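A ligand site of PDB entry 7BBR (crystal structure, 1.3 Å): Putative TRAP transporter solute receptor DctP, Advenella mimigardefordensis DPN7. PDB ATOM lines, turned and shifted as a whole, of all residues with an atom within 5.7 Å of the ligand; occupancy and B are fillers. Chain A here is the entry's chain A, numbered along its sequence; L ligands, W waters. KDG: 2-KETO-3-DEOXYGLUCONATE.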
ATOM      1  N   TYR A  38     -28.771  21.391 -26.288  1.00  0.00           N
ATOM      2  CA  TYR A  38     -29.069  20.127 -26.953  1.00  0.00           C
ATOM      3  C   TYR A  38     -27.752  19.412 -27.274  1.00  0.00           C
ATOM      4  O   TYR A  38     -26.668  19.991 -27.202  1.00  0.00           O
ATOM      5  CB  TYR A  38     -29.961  20.317 -28.187  1.00  0.00           C
ATOM      6  CG  TYR A  38     -29.436  21.268 -29.234  1.00  0.00           C
ATOM      7  CD1 TYR A  38     -28.620  20.808 -30.250  1.00  0.00           C
ATOM      8  CD2 TYR A  38     -29.782  22.587 -29.235  1.00  0.00           C
ATOM      9  CE1 TYR A  38     -28.143  21.629 -31.215  1.00  0.00           C
ATOM     10  CE2 TYR A  38     -29.313  23.438 -30.200  1.00  0.00           C
ATOM     11  CZ  TYR A  38     -28.477  22.953 -31.197  1.00  0.00           C
ATOM     12  OH  TYR A  38     -27.967  23.765 -32.193  1.00  0.00           O
ATOM     13  N   GLY A  39     -27.887  18.135 -27.613  1.00  0.00           N
ATOM     14  CA  GLY A  39     -26.762  17.259 -27.880  1.00  0.00           C
ATOM     15  C   GLY A  39     -26.220  17.246 -29.288  1.00  0.00           C
ATOM     16  O   GLY A  39     -25.011  17.183 -29.485  1.00  0.00           O
ATOM     17  N   LEU A  40     -27.084  17.274 -30.292  1.00  0.00           N
ATOM     18  CA  LEU A  40     -26.653  17.192 -31.677  1.00  0.00           C
ATOM     19  C   LEU A  40     -25.835  18.419 -32.079  1.00  0.00           C
ATOM     20  O   LEU A  40     -25.863  19.468 -31.423  1.00  0.00           O
ATOM     21  CB  LEU A  40     -27.852  17.078 -32.612  1.00  0.00           C
ATOM     22  CG  LEU A  40     -28.730  15.827 -32.531  1.00  0.00           C
ATOM     23  CD1 LEU A  40     -29.688  15.806 -33.708  1.00  0.00           C
ATOM     24  CD2 LEU A  40     -27.882  14.569 -32.502  1.00  0.00           C
ATOM     25  N   PRO A  77     -25.409  16.134 -21.904  1.00  0.00           N
ATOM     26  CA  PRO A  77     -26.222  15.189 -22.672  1.00  0.00           C
ATOM     27  C   PRO A  77     -27.672  15.242 -22.219  1.00  0.00           C
ATOM     28  O   PRO A  77     -28.026  15.923 -21.264  1.00  0.00           O
ATOM     29  CB  PRO A  77     -25.582  13.825 -22.327  1.00  0.00           C
ATOM     30  CG  PRO A  77     -25.087  14.023 -20.898  1.00  0.00           C
ATOM     31  CD  PRO A  77     -24.580  15.463 -20.871  1.00  0.00           C
ATOM     32  N   ASP A  78     -28.497  14.431 -22.894  1.00  0.00           N
ATOM     33  CA  ASP A  78     -29.931  14.404 -22.636  1.00  0.00           C
ATOM     34  C   ASP A  78     -30.247  14.282 -21.152  1.00  0.00           C
ATOM     35  O   ASP A  78     -31.148  14.953 -20.644  1.00  0.00           O
ATOM     36  CB  ASP A  78     -30.588  13.223 -23.369  1.00  0.00           C
ATOM     37  CG  ASP A  78     -30.692  13.397 -24.874  1.00  0.00           C
ATOM     38  OD1 ASP A  78     -30.412  14.488 -25.406  1.00  0.00           O
ATOM     39  OD2 ASP A  78     -31.089  12.387 -25.513  1.00  0.00           O
ATOM     40  N   LEU A  81     -29.699  17.540 -19.526  1.00  0.00           N
ATOM     41  CA  LEU A  81     -30.656  18.528 -20.024  1.00  0.00           C
ATOM     42  C   LEU A  81     -32.024  18.334 -19.380  1.00  0.00           C
ATOM     43  O   LEU A  81     -32.672  19.306 -18.955  1.00  0.00           O
ATOM     44  CB  LEU A  81     -30.755  18.412 -21.551  1.00  0.00           C
ATOM     45  CG  LEU A  81     -29.494  18.826 -22.304  1.00  0.00           C
ATOM     46  CD1 LEU A  81     -29.502  18.271 -23.701  1.00  0.00           C
ATOM     47  CD2 LEU A  81     -29.351  20.348 -22.304  1.00  0.00           C
ATOM     48  N   PHE A  94     -34.555  19.560 -26.583  1.00  0.00           N
ATOM     49  CA  PHE A  94     -35.139  18.389 -27.208  1.00  0.00           C
ATOM     50  C   PHE A  94     -34.251  17.223 -26.800  1.00  0.00           C
ATOM     51  O   PHE A  94     -33.039  17.374 -26.702  1.00  0.00           O
ATOM     52  CB  PHE A  94     -35.300  18.497 -28.748  1.00  0.00           C
ATOM     53  CG  PHE A  94     -33.997  18.608 -29.489  1.00  0.00           C
ATOM     54  CD1 PHE A  94     -33.287  17.478 -29.872  1.00  0.00           C
ATOM     55  CD2 PHE A  94     -33.493  19.847 -29.842  1.00  0.00           C
ATOM     56  CE1 PHE A  94     -32.078  17.587 -30.566  1.00  0.00           C
ATOM     57  CE2 PHE A  94     -32.296  19.961 -30.519  1.00  0.00           C
ATOM     58  CZ  PHE A  94     -31.590  18.837 -30.894  1.00  0.00           C
ATOM     59  N   VAL A  95     -34.869  16.077 -26.495  1.00  0.00           N
ATOM     60  CA  VAL A  95     -34.152  14.861 -26.131  1.00  0.00           C
ATOM     61  C   VAL A  95     -34.813  13.677 -26.805  1.00  0.00           C
ATOM     62  O   VAL A  95     -35.988  13.719 -27.151  1.00  0.00           O
ATOM     63  CB  VAL A  95     -34.092  14.633 -24.606  1.00  0.00           C
ATOM     64  CG1 VAL A  95     -33.345  15.765 -23.922  1.00  0.00           C
ATOM     65  CG2 VAL A  95     -35.489  14.400 -24.032  1.00  0.00           C
ATOM     66  N   SER A  96     -34.063  12.593 -26.957  1.00  0.00           N
ATOM     67  CA  SER A  96     -34.667  11.356 -27.406  1.00  0.00           C
ATOM     68  C   SER A  96     -35.594  10.798 -26.315  1.00  0.00           C
ATOM     69  O   SER A  96     -35.446  11.088 -25.128  1.00  0.00           O
ATOM     70  CB  SER A  96     -33.586  10.329 -27.759  1.00  0.00           C
ATOM     71  OG  SER A  96     -32.903  10.689 -28.955  1.00  0.00           O
ATOM     72  N   PRO A  99     -33.915   8.262 -22.955  1.00  0.00           N
ATOM     73  CA  PRO A  99     -33.543   8.656 -21.580  1.00  0.00           C
ATOM     74  C   PRO A  99     -34.746   9.008 -20.729  1.00  0.00           C
ATOM     75  O   PRO A  99     -34.641   8.995 -19.495  1.00  0.00           O
ATOM     76  CB  PRO A  99     -32.590   9.841 -21.778  1.00  0.00           C
ATOM     77  CG  PRO A  99     -32.912  10.377 -23.174  1.00  0.00           C
ATOM     78  CD  PRO A  99     -33.255   9.128 -23.965  1.00  0.00           C
ATOM     79  N   ASN A 151     -36.190  12.479 -34.456  1.00  0.00           N
ATOM     80  CA  ASN A 151     -34.792  12.059 -34.492  1.00  0.00           C
ATOM     81  C   ASN A 151     -34.629  11.191 -35.732  1.00  0.00           C
ATOM     82  O   ASN A 151     -34.004  11.599 -36.715  1.00  0.00           O
ATOM     83  CB  ASN A 151     -34.417  11.412 -33.156  1.00  0.00           C
ATOM     84  CG  ASN A 151     -32.943  11.074 -33.043  1.00  0.00           C
ATOM     85  OD1 ASN A 151     -32.178  11.247 -33.985  1.00  0.00           O
ATOM     86  ND2 ASN A 151     -32.547  10.564 -31.871  1.00  0.00           N
ATOM     87  N   ARG A 154     -32.928   4.734 -37.206  1.00  0.00           N
ATOM     88  CA  ARG A 154     -31.548   4.506 -36.781  1.00  0.00           C
ATOM     89  C   ARG A 154     -30.887   3.448 -37.661  1.00  0.00           C
ATOM     90  O   ARG A 154     -31.516   2.481 -38.098  1.00  0.00           O
ATOM     91  CB  ARG A 154     -31.537   4.072 -35.309  1.00  0.00           C
ATOM     92  CG  ARG A 154     -32.304   5.025 -34.401  1.00  0.00           C
ATOM     93  CD  ARG A 154     -32.318   4.568 -32.968  1.00  0.00           C
ATOM     94  NE  ARG A 154     -31.021   4.847 -32.321  1.00  0.00           N
ATOM     95  CZ  ARG A 154     -30.711   5.971 -31.715  1.00  0.00           C
ATOM     96  NH1 ARG A 154     -31.591   6.969 -31.655  1.00  0.00           N
ATOM     97  NH2 ARG A 154     -29.500   6.107 -31.198  1.00  0.00           N
ATOM     98  N   ARG A 175     -22.337   0.629 -28.869  1.00  0.00           N
ATOM     99  CA  ARG A 175     -22.953   1.590 -27.965  1.00  0.00           C
ATOM    100  C   ARG A 175     -24.443   1.655 -28.243  1.00  0.00           C
ATOM    101  O   ARG A 175     -24.870   1.661 -29.402  1.00  0.00           O
ATOM    102  CB  ARG A 175     -22.319   2.972 -28.147  1.00  0.00           C
ATOM    103  CG  ARG A 175     -22.981   4.045 -27.265  1.00  0.00           C
ATOM    104  CD  ARG A 175     -24.182   4.707 -27.960  1.00  0.00           C
ATOM    105  NE  ARG A 175     -24.741   5.803 -27.167  1.00  0.00           N
ATOM    106  CZ  ARG A 175     -25.726   6.569 -27.592  1.00  0.00           C
ATOM    107  NH1 ARG A 175     -26.242   6.340 -28.804  1.00  0.00           N
ATOM    108  NH2 ARG A 175     -26.204   7.556 -26.830  1.00  0.00           N
ATOM    109  N   MET A 177     -28.308   3.520 -26.518  1.00  0.00           N
ATOM    110  CA  MET A 177     -28.900   4.495 -25.611  1.00  0.00           C
ATOM    111  C   MET A 177     -29.166   3.864 -24.250  1.00  0.00           C
ATOM    112  O   MET A 177     -29.155   2.644 -24.087  1.00  0.00           O
ATOM    113  CB  MET A 177     -30.142   5.114 -26.221  1.00  0.00           C
ATOM    114  CG  MET A 177     -29.857   5.998 -27.426  1.00  0.00           C
ATOM    115  SD  MET A 177     -31.246   6.963 -28.046  1.00  0.00           S
ATOM    116  CE  MET A 177     -32.266   5.662 -28.718  1.00  0.00           C
ATOM    117  N   MET A 196     -24.188   4.307 -23.248  1.00  0.00           N
ATOM    118  CA  MET A 196     -23.302   5.437 -23.045  1.00  0.00           C
ATOM    119  C   MET A 196     -24.035   6.725 -23.409  1.00  0.00           C
ATOM    120  O   MET A 196     -24.817   6.716 -24.361  1.00  0.00           O
ATOM    121  CB  MET A 196     -22.075   5.385 -23.967  1.00  0.00           C
ATOM    122  CG  MET A 196     -21.186   4.196 -23.843  1.00  0.00           C
ATOM    123  SD  MET A 196     -19.748   4.335 -24.949  1.00  0.00           S
ATOM    124  CE  MET A 196     -19.784   6.050 -25.325  1.00  0.00           C
ATOM    125  N   PRO A 197     -23.778   7.826 -22.714  1.00  0.00           N
ATOM    126  CA  PRO A 197     -24.340   9.115 -23.165  1.00  0.00           C
ATOM    127  C   PRO A 197     -23.804   9.504 -24.533  1.00  0.00           C
ATOM    128  O   PRO A 197     -22.647   9.245 -24.881  1.00  0.00           O
ATOM    129  CB  PRO A 197     -23.879  10.108 -22.096  1.00  0.00           C
ATOM    130  CG  PRO A 197     -23.045   9.417 -21.160  1.00  0.00           C
ATOM    131  CD  PRO A 197     -22.894   7.989 -21.530  1.00  0.00           C
ATOM    132  N   PHE A 198     -24.661  10.193 -25.293  1.00  0.00           N
ATOM    133  CA  PHE A 198     -24.325  10.577 -26.674  1.00  0.00           C
ATOM    134  C   PHE A 198     -23.095  11.464 -26.724  1.00  0.00           C
ATOM    135  O   PHE A 198     -22.305  11.394 -27.672  1.00  0.00           O
ATOM    136  CB  PHE A 198     -25.514  11.326 -27.248  1.00  0.00           C
ATOM    137  CG  PHE A 198     -25.330  11.766 -28.666  1.00  0.00           C
ATOM    138  CD1 PHE A 198     -25.526  10.863 -29.713  1.00  0.00           C
ATOM    139  CD2 PHE A 198     -24.973  13.069 -28.973  1.00  0.00           C
ATOM    140  CE1 PHE A 198     -25.357  11.256 -31.028  1.00  0.00           C
ATOM    141  CE2 PHE A 198     -24.796  13.461 -30.282  1.00  0.00           C
ATOM    142  CZ  PHE A 198     -24.997  12.547 -31.308  1.00  0.00           C
ATOM    143  N   LEU A 201     -19.778   9.728 -27.290  1.00  0.00           N
ATOM    144  CA  LEU A 201     -19.799   8.702 -28.329  1.00  0.00           C
ATOM    145  C   LEU A 201     -18.695   8.882 -29.351  1.00  0.00           C
ATOM    146  O   LEU A 201     -18.027   7.907 -29.719  1.00  0.00           O
ATOM    147  CB  LEU A 201     -21.186   8.678 -28.962  1.00  0.00           C
ATOM    148  CG  LEU A 201     -21.446   7.584 -29.984  1.00  0.00           C
ATOM    149  CD1 LEU A 201     -20.974   6.218 -29.505  1.00  0.00           C
ATOM    150  CD2 LEU A 201     -22.936   7.608 -30.268  1.00  0.00           C
ATOM    151  N   GLN A 213     -22.084   1.991 -33.209  1.00  0.00           N
ATOM    152  CA  GLN A 213     -23.238   2.644 -32.605  1.00  0.00           C
ATOM    153  C   GLN A 213     -24.363   2.589 -33.635  1.00  0.00           C
ATOM    154  O   GLN A 213     -24.221   1.970 -34.698  1.00  0.00           O
ATOM    155  CB  GLN A 213     -22.900   4.078 -32.181  1.00  0.00           C
ATOM    156  CG  GLN A 213     -22.492   4.996 -33.328  1.00  0.00           C
ATOM    157  CD  GLN A 213     -23.644   5.633 -34.045  1.00  0.00           C
ATOM    158  OE1 GLN A 213     -24.483   6.307 -33.431  1.00  0.00           O
ATOM    159  NE2 GLN A 213     -23.731   5.427 -35.341  1.00  0.00           N
ATOM    160  N   GLU A 214     -25.472   3.260 -33.339  1.00  0.00           N
ATOM    161  CA  GLU A 214     -26.585   3.309 -34.263  1.00  0.00           C
ATOM    162  C   GLU A 214     -27.340   4.619 -34.049  1.00  0.00           C
ATOM    163  O   GLU A 214     -27.596   5.024 -32.913  1.00  0.00           O
ATOM    164  CB  GLU A 214     -27.500   2.062 -34.164  1.00  0.00           C
ATOM    165  CG  GLU A 214     -27.844   1.573 -32.755  1.00  0.00           C
ATOM    166  CD  GLU A 214     -29.011   2.308 -32.172  1.00  0.00           C
ATOM    167  OE1 GLU A 214     -28.785   2.926 -31.092  1.00  0.00           O
ATOM    168  OE2 GLU A 214     -30.132   2.224 -32.739  1.00  0.00           O
ATOM    169  N   ASN A 215     -27.650   5.298 -35.157  1.00  0.00           N
ATOM    170  CA  ASN A 215     -28.245   6.631 -35.114  1.00  0.00           C
ATOM    171  C   ASN A 215     -28.726   6.961 -36.528  1.00  0.00           C
ATOM    172  O   ASN A 215     -28.343   6.260 -37.493  1.00  0.00           O
ATOM    173  CB  ASN A 215     -27.236   7.703 -34.657  1.00  0.00           C
ATOM    174  CG  ASN A 215     -27.489   8.214 -33.263  1.00  0.00           C
ATOM    175  OD1 ASN A 215     -28.516   8.834 -33.004  1.00  0.00           O
ATOM    176  ND2 ASN A 215     -26.567   7.960 -32.362  1.00  0.00           N
ATOM    177  N   PRO A 216     -29.532   8.001 -36.706  1.00  0.00           N
ATOM    178  CA  PRO A 216     -29.923   8.407 -38.060  1.00  0.00           C
ATOM    179  C   PRO A 216     -28.723   8.892 -38.854  1.00  0.00           C
ATOM    180  O   PRO A 216     -27.733   9.382 -38.311  1.00  0.00           O
ATOM    181  CB  PRO A 216     -30.943   9.517 -37.816  1.00  0.00           C
ATOM    182  CG  PRO A 216     -31.500   9.230 -36.419  1.00  0.00           C
ATOM    183  CD  PRO A 216     -30.287   8.739 -35.677  1.00  0.00           C
ATOM    184  N   THR A 240     -36.679   6.742 -33.534  1.00  0.00           N
ATOM    185  CA  THR A 240     -36.625   7.520 -32.304  1.00  0.00           C
ATOM    186  C   THR A 240     -37.343   8.846 -32.473  1.00  0.00           C
ATOM    187  O   THR A 240     -36.907   9.670 -33.291  1.00  0.00           O
ATOM    188  CB  THR A 240     -35.182   7.762 -31.856  1.00  0.00           C
ATOM    189  OG1 THR A 240     -34.529   6.510 -31.703  1.00  0.00           O
ATOM    190  CG2 THR A 240     -35.137   8.539 -30.543  1.00  0.00           C
ATOM    191  N   PHE A 242     -37.927  12.602 -30.968  1.00  0.00           N
ATOM    192  CA  PHE A 242     -37.514  13.562 -29.957  1.00  0.00           C
ATOM    193  C   PHE A 242     -38.766  14.100 -29.268  1.00  0.00           C
ATOM    194  O   PHE A 242     -39.819  14.262 -29.892  1.00  0.00           O
ATOM    195  CB  PHE A 242     -36.822  14.767 -30.603  1.00  0.00           C
ATOM    196  CG  PHE A 242     -35.412  14.531 -31.082  1.00  0.00           C
ATOM    197  CD1 PHE A 242     -34.461  13.876 -30.310  1.00  0.00           C
ATOM    198  CD2 PHE A 242     -35.024  15.027 -32.326  1.00  0.00           C
ATOM    199  CE1 PHE A 242     -33.149  13.748 -30.752  1.00  0.00           C
ATOM    200  CE2 PHE A 242     -33.712  14.913 -32.766  1.00  0.00           C
ATOM    201  CZ  PHE A 242     -32.781  14.250 -31.983  1.00  0.00           C
HETATM  202  O1B KDG L   1     -29.454  15.901 -29.238  1.00  0.00           O
HETATM  203  C1  KDG L   1     -29.912  14.557 -29.319  1.00  0.00           C
HETATM  204  C2  KDG L   1     -28.915  13.621 -28.624  1.00  0.00           C
HETATM  205  O2  KDG L   1     -28.612  14.108 -27.327  1.00  0.00           O
HETATM  206  C3  KDG L   1     -29.401  12.173 -28.472  1.00  0.00           C
HETATM  207  O3  KDG L   1     -30.749  12.174 -28.086  1.00  0.00           O
HETATM  208  C4  KDG L   1     -29.332  11.438 -29.782  1.00  0.00           C
HETATM  209  O5  KDG L   1     -30.080   9.444 -30.838  1.00  0.00           O
HETATM  210  C5  KDG L   1     -29.548   9.939 -29.831  1.00  0.00           C
HETATM  211  C6  KDG L   1     -28.596   9.063 -29.027  1.00  0.00           C
HETATM  212  O6A KDG L   1     -27.948   8.273 -29.755  1.00  0.00           O
HETATM  213  O6B KDG L   1     -28.370   9.168 -27.807  1.00  0.00           O
HETATM  214  O   HOH W   1     -29.718   9.813 -25.541  1.00  0.00           O
HETATM  215  O   HOH W   2     -29.506  11.483 -33.525  1.00  0.00           O
HETATM  216  O   HOH W   3     -30.416  16.883 -26.889  1.00  0.00           O
HETATM  217  O   HOH W   4     -27.189  13.336 -25.127  1.00  0.00           O
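The side-chain sulfur (SD) of Met 177 lies close to an oxygen (O6B) of the ligand (3.6 Å).
Residues that only touch the ligand: Phe 94, Phe 198 and Phe 242.
Hydrophobic or aromatic side chains within 4 Å of the ligand: Leu 40, Phe 94, Met 177, Phe 198 and Phe 242.
Water W1 lies within hydrogen-bond range of O6B of the ligand (2.7 Å) and OD2 of Asp 78 (2.9 Å).
Water W3 lies within hydrogen-bond range of O of Phe 94, O1B of the ligand, OD1 of Asp 78 and N of Gly 39.
Water W4 bridges O2 of the ligand (2.7 Å) and N of Asp 78 (2.8 Å).
The guanidinium group (NH2) of Arg 154 lies within salt-bridge range of an oxygen (O6A) of the ligand, 3.0 Å away.
The guanidinium group (NH1) of Arg 175 lies within salt-bridge range of an oxygen (O6A) of the ligand, at 2.7 Å.
The side-chain amide oxygen (OD1) of Asn 215 lies close to an oxygen (O5) of the ligand.
N of Gly 39 lies within hydrogen-bond range of O1B of the ligand, at 3.2 Å.
An oxygen (O3) of the ligand is in hydrogen-bond range of the side-chain hydroxyl (OG) of Ser 96 (2.8 Å).
The side-chain amide nitrogen (ND2) of Asn 151 sits at hydrogen-bond distance from an oxygen (O5) of the ligand (2.9 Å).
OD2 of Asp 78 lies within hydrogen-bond range of O3 of the ligand, 2.6 Å away.
O1B of the ligand lies within hydrogen-bond range of N of Leu 40 (2.9 Å).
The side-chain amide nitrogen (ND2) of Asn 215 sits at hydrogen-bond distance from the side-chain amide oxygen (OE1) of Gln 213.
NH1 of Arg 154 is in hydrogen-bond range of OG1 of Thr 240, 3.0 Å away.
The side-chain hydroxyl (OG) of Ser 96 is in hydrogen-bond range of the side-chain amide nitrogen (ND2) of Asn 151 (2.9 Å).
The backbone carbonyl oxygen of Thr 240 sits close to the backbone NH of Asn 151 (3.1 Å).
NE of Arg 175 lies within hydrogen-bond range of O of Met 196 (3.0 Å).
The side-chain carboxylate (OE2) of Glu 214 lies within salt-bridge range of the guanidinium group (NE) of Arg 154, 2.8 Å away.
The side-chain amide oxygen (OD1) of Asn 215 lies within hydrogen-bond range of the guanidinium group (NH2) of Arg 154, 3.4 Å away.
OD2 of Asp 78 sits at hydrogen-bond distance from N of Ser 96 (3.3 Å).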
